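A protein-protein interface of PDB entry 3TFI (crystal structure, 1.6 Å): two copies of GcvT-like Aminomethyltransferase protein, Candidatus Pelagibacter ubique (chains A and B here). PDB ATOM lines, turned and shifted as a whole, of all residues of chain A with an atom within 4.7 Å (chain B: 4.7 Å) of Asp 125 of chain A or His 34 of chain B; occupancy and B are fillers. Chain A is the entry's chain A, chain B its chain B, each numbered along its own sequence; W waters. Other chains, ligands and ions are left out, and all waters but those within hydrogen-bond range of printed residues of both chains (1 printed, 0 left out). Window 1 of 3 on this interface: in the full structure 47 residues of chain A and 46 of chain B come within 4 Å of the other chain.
The backbone carbonyl oxygen (O) of Ile 31 of chain A is in hydrogen-bond range of the guanidinium group (NH1) of Arg 11 of chain B (2.8 Å). The side-chain carboxylate (OD2) of Asp 125 of chain A lies within hydrogen-bond range of a ring nitrogen (NE2) of His 34 of chain B (3.2 Å). NH1 of Arg 11 of chain B lies within salt-bridge range of OD1 of Asp 125 of chain A (2.8 Å).
The side-chain hydroxyl (OG) of Ser 126 of chain A is in hydrogen-bond range of the side-chain amide nitrogen (ND2) of Asn 107 of chain A. N of Asn 33 of chain A sits at hydrogen-bond distance from OD2 of Asp 125 of chain A, 2.8 Å away. O of His 34 of chain B sits at hydrogen-bond distance from NE of Arg 13 of chain B (3.0 Å). OD1 of Asp 127 of chain B sits close to ND1 of His 34 of chain B. The backbone NH (N) of Ser 126 of chain A sits at hydrogen-bond distance from the side-chain amide oxygen (OD1) of Asn 33 of chain A.
Among the printed residues, pairs that only touch across the chains: Ile 31 of chain A with Leu 12 of chain B (3.8 Å), Ile 31 of chain A with Ile 31 of chain B (3.7 Å), Tyr 32 of chain A with Arg 11 of chain B (3.7 Å), Ser 126 of chain A with Asp 127 of chain B (3.4 Å) and Tyr 247 of chain A with Arg 11 of chain B (3.2 Å).
Of the printed residues of chain B, Tyr 32 of chain A touches Arg 11 (3.7 Å). Asn 33 of chain A touches none of the printed residues of chain B. Of the printed residues of chain B, Ser 126 of chain A touches Asp 127. His 34 of chain B touches just one residue of chain A: Asp 125 (3.0 Å). Of the printed residues of chain A, Asp 127 of chain B touches Ser 126 (3.4 Å). The nearest residue of chain A that does not touch His 34 of chain B is Ser 126 of chain A (4.1 Å).
Of the 10 printed residues of chain B, 5 touch a printed residue of chain A. Hydrophobic or aromatic side chains of chain B within 4 Å of the printed part of chain A: Leu 12, Ile 31 and His 34. Of the 9 printed residues of chain A, 5 touch a printed residue of chain B. Among the printed residues, 8 pairs touch across the chains. Among the printed residues, Asp or Glu carboxylates within 4 Å of a Lys or Arg side-chain nitrogen of the other chain: Asp 125 of chain A with Arg 11 of chain B.
Ile 31 of chain B touches its own counterpart, Ile 31 of chain A. Positions printed for both chains: 31, 32 and 33. Of the 8 pairs that touch across the chains among the printed residues, 1 has its exchanged pair printed and touching as well.
Water W1 lies within hydrogen-bond range of the side-chain amide oxygen of Asn 33 of chain A (2.9 Å), a ring nitrogen (NE2) of His 34 of chain B (3.1 Å), the side-chain carboxylate of Asp 125 of chain A (3.4 Å) and the backbone NH of Ser 126 of chain A (3.4 Å).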
ATOM      1  N   ILE A  31      17.775   9.946  21.353  1.00  0.00           N
ATOM      2  CA  ILE A  31      18.512   8.718  21.540  1.00  0.00           C
ATOM      3  C   ILE A  31      19.931   8.951  21.074  1.00  0.00           C
ATOM      4  O   ILE A  31      20.141   9.515  20.004  1.00  0.00           O
ATOM      5  CB  ILE A  31      17.903   7.532  20.747  1.00  0.00           C
ATOM      6  CG1 ILE A  31      16.492   7.220  21.281  1.00  0.00           C
ATOM      7  CG2 ILE A  31      18.746   6.262  20.791  1.00  0.00           C
ATOM      8  CD1 ILE A  31      16.385   6.856  22.742  1.00  0.00           C
ATOM      9  N   TYR A  32      20.877   8.490  21.869  1.00  0.00           N
ATOM     10  CA  TYR A  32      22.299   8.770  21.618  1.00  0.00           C
ATOM     11  C   TYR A  32      23.032   7.510  22.078  1.00  0.00           C
ATOM     12  O   TYR A  32      22.864   7.080  23.199  1.00  0.00           O
ATOM     13  CB  TYR A  32      22.673  10.007  22.390  1.00  0.00           C
ATOM     14  CG  TYR A  32      23.958  10.691  22.132  1.00  0.00           C
ATOM     15  CD1 TYR A  32      24.005  11.845  21.387  1.00  0.00           C
ATOM     16  CD2 TYR A  32      25.112  10.266  22.706  1.00  0.00           C
ATOM     17  CE1 TYR A  32      25.171  12.506  21.178  1.00  0.00           C
ATOM     18  CE2 TYR A  32      26.301  10.936  22.501  1.00  0.00           C
ATOM     19  CZ  TYR A  32      26.330  12.045  21.732  1.00  0.00           C
ATOM     20  OH  TYR A  32      27.537  12.744  21.616  1.00  0.00           O
ATOM     21  N   ASN A  33      23.805   6.871  21.203  1.00  0.00           N
ATOM     22  CA  ASN A  33      24.407   5.611  21.547  1.00  0.00           C
ATOM     23  C   ASN A  33      23.436   4.595  22.144  1.00  0.00           C
ATOM     24  O   ASN A  33      23.699   3.981  23.189  1.00  0.00           O
ATOM     25  CB  ASN A  33      25.622   5.817  22.488  1.00  0.00           C
ATOM     26  CG  ASN A  33      26.793   6.436  21.785  1.00  0.00           C
ATOM     27  OD1 ASN A  33      27.187   5.982  20.696  1.00  0.00           O
ATOM     28  ND2 ASN A  33      27.378   7.443  22.399  1.00  0.00           N
ATOM     29  N   ASN A 107      33.690   9.703  14.550  1.00  0.00           N
ATOM     30  CA  ASN A 107      33.244  10.120  15.893  1.00  0.00           C
ATOM     31  C   ASN A 107      34.214  11.222  16.275  1.00  0.00           C
ATOM     32  O   ASN A 107      35.310  11.261  15.705  1.00  0.00           O
ATOM     33  CB  ASN A 107      33.374   8.928  16.846  1.00  0.00           C
ATOM     34  CG  ASN A 107      32.522   9.055  18.114  1.00  0.00           C
ATOM     35  OD1 ASN A 107      32.943   9.704  19.083  1.00  0.00           O
ATOM     36  ND2 ASN A 107      31.327   8.373  18.136  1.00  0.00           N
ATOM     37  N   ILE A 123      32.533   8.847  23.952  1.00  0.00           N
ATOM     38  CA  ILE A 123      32.144   8.897  22.529  1.00  0.00           C
ATOM     39  C   ILE A 123      30.884   9.730  22.210  1.00  0.00           C
ATOM     40  O   ILE A 123      29.953   9.898  23.024  1.00  0.00           O
ATOM     41  CB  ILE A 123      32.010   7.492  21.969  1.00  0.00           C
ATOM     42  CG1 ILE A 123      30.936   6.658  22.651  1.00  0.00           C
ATOM     43  CG2 ILE A 123      33.370   6.725  21.929  1.00  0.00           C
ATOM     44  CD1 ILE A 123      30.436   5.427  21.840  1.00  0.00           C
ATOM     45  N   ALA A 124      30.876  10.291  21.018  1.00  0.00           N
ATOM     46  CA  ALA A 124      29.669  10.856  20.365  1.00  0.00           C
ATOM     47  C   ALA A 124      28.819   9.697  19.805  1.00  0.00           C
ATOM     48  O   ALA A 124      29.035   8.554  20.160  1.00  0.00           O
ATOM     49  CB  ALA A 124      30.101  11.807  19.262  1.00  0.00           C
ATOM     50  N   ASP A 125      27.783   9.997  19.030  1.00  0.00           N
ATOM     51  CA  ASP A 125      26.777   8.993  18.650  1.00  0.00           C
ATOM     52  C   ASP A 125      27.148   8.051  17.463  1.00  0.00           C
ATOM     53  O   ASP A 125      26.611   8.171  16.341  1.00  0.00           O
ATOM     54  CB  ASP A 125      25.493   9.725  18.348  1.00  0.00           C
ATOM     55  CG  ASP A 125      24.304   8.795  18.014  1.00  0.00           C
ATOM     56  OD1 ASP A 125      23.440   9.234  17.151  1.00  0.00           O
ATOM     57  OD2 ASP A 125      24.226   7.684  18.587  1.00  0.00           O
ATOM     58  N   SER A 126      28.083   7.156  17.741  1.00  0.00           N
ATOM     59  CA  SER A 126      28.395   6.036  16.837  1.00  0.00           C
ATOM     60  C   SER A 126      29.102   4.935  17.598  1.00  0.00           C
ATOM     61  O   SER A 126      29.724   5.204  18.640  1.00  0.00           O
ATOM     62  CB  SER A 126      29.211   6.435  15.648  1.00  0.00           C
ATOM     63  OG  SER A 126      30.543   6.793  15.927  1.00  0.00           O
ATOM     64  N   TYR A 247      28.422  15.105  15.987  1.00  0.00           N
ATOM     65  CA  TYR A 247      28.517  14.072  14.999  1.00  0.00           C
ATOM     66  C   TYR A 247      27.142  13.551  14.662  1.00  0.00           C
ATOM     67  O   TYR A 247      26.325  13.251  15.542  1.00  0.00           O
ATOM     68  CB  TYR A 247      29.365  12.889  15.497  1.00  0.00           C
ATOM     69  CG  TYR A 247      29.451  11.763  14.485  1.00  0.00           C
ATOM     70  CD1 TYR A 247      30.283  11.860  13.392  1.00  0.00           C
ATOM     71  CD2 TYR A 247      28.581  10.639  14.554  1.00  0.00           C
ATOM     72  CE1 TYR A 247      30.280  10.835  12.414  1.00  0.00           C
ATOM     73  CE2 TYR A 247      28.561   9.694  13.566  1.00  0.00           C
ATOM     74  CZ  TYR A 247      29.423   9.764  12.535  1.00  0.00           C
ATOM     75  OH  TYR A 247      29.365   8.730  11.597  1.00  0.00           O
ATOM     76  N   ARG B  11      20.476  14.325  13.066  1.00  0.00           N
ATOM     77  CA  ARG B  11      21.124  13.105  13.544  1.00  0.00           C
ATOM     78  C   ARG B  11      20.162  11.940  13.701  1.00  0.00           C
ATOM     79  O   ARG B  11      20.561  10.783  13.519  1.00  0.00           O
ATOM     80  CB  ARG B  11      21.830  13.429  14.859  1.00  0.00           C
ATOM     81  CG  ARG B  11      22.584  12.339  15.484  1.00  0.00           C
ATOM     82  CD  ARG B  11      23.398  12.767  16.729  1.00  0.00           C
ATOM     83  NE  ARG B  11      22.493  13.223  17.797  1.00  0.00           N
ATOM     84  CZ  ARG B  11      21.733  12.451  18.540  1.00  0.00           C
ATOM     85  NH1 ARG B  11      21.749  11.135  18.394  1.00  0.00           N
ATOM     86  NH2 ARG B  11      20.895  13.022  19.368  1.00  0.00           N
ATOM     87  N   LEU B  12      18.929  12.219  14.086  1.00  0.00           N
ATOM     88  CA  LEU B  12      17.867  11.196  14.104  1.00  0.00           C
ATOM     89  C   LEU B  12      17.225  11.178  12.721  1.00  0.00           C
ATOM     90  O   LEU B  12      16.248  11.858  12.432  1.00  0.00           O
ATOM     91  CB  LEU B  12      16.824  11.507  15.156  1.00  0.00           C
ATOM     92  CG  LEU B  12      17.263  11.437  16.617  1.00  0.00           C
ATOM     93  CD1 LEU B  12      16.064  11.441  17.615  1.00  0.00           C
ATOM     94  CD2 LEU B  12      18.237  10.415  16.897  1.00  0.00           C
ATOM     95  N   ARG B  13      17.846  10.433  11.847  1.00  0.00           N
ATOM     96  CA  ARG B  13      17.595  10.613  10.432  1.00  0.00           C
ATOM     97  C   ARG B  13      16.158  10.308  10.028  1.00  0.00           C
ATOM     98  O   ARG B  13      15.592   9.311  10.428  1.00  0.00           O
ATOM     99  CB  ARG B  13      18.512   9.767   9.597  1.00  0.00           C
ATOM    100  CG  ARG B  13      20.018  10.119   9.772  1.00  0.00           C
ATOM    101  CD  ARG B  13      20.912   9.189   8.917  1.00  0.00           C
ATOM    102  NE  ARG B  13      20.940   7.885   9.490  1.00  0.00           N
ATOM    103  CZ  ARG B  13      21.609   6.846   8.933  1.00  0.00           C
ATOM    104  NH1 ARG B  13      22.221   6.976   7.759  1.00  0.00           N
ATOM    105  NH2 ARG B  13      21.563   5.667   9.538  1.00  0.00           N
ATOM    106  N   ILE B  31      14.208   4.716  17.611  1.00  0.00           N
ATOM    107  CA  ILE B  31      15.397   5.042  16.847  1.00  0.00           C
ATOM    108  C   ILE B  31      16.154   3.748  16.666  1.00  0.00           C
ATOM    109  O   ILE B  31      16.297   2.964  17.625  1.00  0.00           O
ATOM    110  CB  ILE B  31      16.284   6.072  17.508  1.00  0.00           C
ATOM    111  CG1 ILE B  31      15.561   7.426  17.656  1.00  0.00           C
ATOM    112  CG2 ILE B  31      17.699   6.263  16.764  1.00  0.00           C
ATOM    113  CD1 ILE B  31      15.244   8.020  16.264  1.00  0.00           C
ATOM    114  N   TYR B  32      16.529   3.513  15.400  1.00  0.00           N
ATOM    115  CA  TYR B  32      17.150   2.251  15.008  1.00  0.00           C
ATOM    116  C   TYR B  32      18.188   2.586  13.970  1.00  0.00           C
ATOM    117  O   TYR B  32      17.883   3.272  12.997  1.00  0.00           O
ATOM    118  CB  TYR B  32      16.046   1.368  14.438  1.00  0.00           C
ATOM    119  CG  TYR B  32      16.302  -0.110  14.263  1.00  0.00           C
ATOM    120  CD1 TYR B  32      15.852  -1.022  15.190  1.00  0.00           C
ATOM    121  CD2 TYR B  32      16.910  -0.612  13.145  1.00  0.00           C
ATOM    122  CE1 TYR B  32      16.040  -2.370  14.998  1.00  0.00           C
ATOM    123  CE2 TYR B  32      17.104  -1.946  12.975  1.00  0.00           C
ATOM    124  CZ  TYR B  32      16.652  -2.835  13.886  1.00  0.00           C
ATOM    125  OH  TYR B  32      16.794  -4.180  13.614  1.00  0.00           O
ATOM    126  N   ASN B  33      19.454   2.210  14.197  1.00  0.00           N
ATOM    127  CA  ASN B  33      20.498   2.705  13.291  1.00  0.00           C
ATOM    128  C   ASN B  33      20.465   4.192  13.035  1.00  0.00           C
ATOM    129  O   ASN B  33      20.604   4.629  11.914  1.00  0.00           O
ATOM    130  CB  ASN B  33      20.501   1.889  12.011  1.00  0.00           C
ATOM    131  CG  ASN B  33      20.975   0.452  12.237  1.00  0.00           C
ATOM    132  OD1 ASN B  33      21.979   0.227  12.914  1.00  0.00           O
ATOM    133  ND2 ASN B  33      20.252  -0.505  11.696  1.00  0.00           N
ATOM    134  N   HIS B  34      20.313   4.975  14.093  1.00  0.00           N
ATOM    135  CA  HIS B  34      20.400   6.405  13.925  1.00  0.00           C
ATOM    136  C   HIS B  34      19.379   6.947  12.930  1.00  0.00           C
ATOM    137  O   HIS B  34      19.618   7.926  12.235  1.00  0.00           O
ATOM    138  CB  HIS B  34      21.838   6.876  13.535  1.00  0.00           C
ATOM    139  CG  HIS B  34      22.901   6.282  14.353  1.00  0.00           C
ATOM    140  ND1 HIS B  34      23.726   5.249  13.969  1.00  0.00           N
ATOM    141  CD2 HIS B  34      23.297   6.631  15.591  1.00  0.00           C
ATOM    142  CE1 HIS B  34      24.581   4.997  14.966  1.00  0.00           C
ATOM    143  NE2 HIS B  34      24.366   5.842  15.927  1.00  0.00           N
ATOM    144  N   MET B  35      18.213   6.327  12.958  1.00  0.00           N
ATOM    145  CA  MET B  35      17.146   6.631  12.008  1.00  0.00           C
ATOM    146  C   MET B  35      15.775   6.387  12.660  1.00  0.00           C
ATOM    147  O   MET B  35      15.610   5.483  13.481  1.00  0.00           O
ATOM    148  CB  MET B  35      17.325   5.838  10.722  1.00  0.00           C
ATOM    149  CG  MET B  35      16.318   6.173   9.660  1.00  0.00           C
ATOM    150  SD  MET B  35      16.772   5.425   8.030  1.00  0.00           S
ATOM    151  CE  MET B  35      18.136   6.504   7.595  1.00  0.00           C
ATOM    152  N   LEU B  36      14.814   7.238  12.303  1.00  0.00           N
ATOM    153  CA  LEU B  36      13.465   7.113  12.768  1.00  0.00           C
ATOM    154  C   LEU B  36      12.842   5.819  12.222  1.00  0.00           C
ATOM    155  O   LEU B  36      12.871   5.568  11.006  1.00  0.00           O
ATOM    156  CB  LEU B  36      12.607   8.316  12.324  1.00  0.00           C
ATOM    157  CG  LEU B  36      12.939   9.682  12.996  1.00  0.00           C
ATOM    158  CD1 LEU B  36      12.267  10.806  12.120  1.00  0.00           C
ATOM    159  CD2 LEU B  36      12.491   9.649  14.414  1.00  0.00           C
ATOM    160  N   ASP B 127      26.264  -0.432  14.565  1.00  0.00           N
ATOM    161  CA  ASP B 127      27.012   0.137  13.456  1.00  0.00           C
ATOM    162  C   ASP B 127      28.019  -0.851  12.890  1.00  0.00           C
ATOM    163  O   ASP B 127      29.267  -0.621  12.986  1.00  0.00           O
ATOM    164  CB  ASP B 127      27.687   1.471  13.800  1.00  0.00           C
ATOM    165  CG  ASP B 127      26.675   2.571  14.212  1.00  0.00           C
ATOM    166  OD1 ASP B 127      25.509   2.543  13.727  1.00  0.00           O
ATOM    167  OD2 ASP B 127      27.054   3.484  14.985  1.00  0.00           O
HETATM  168  O   HOH W   1      25.815   4.705  18.470  1.00  0.00           O
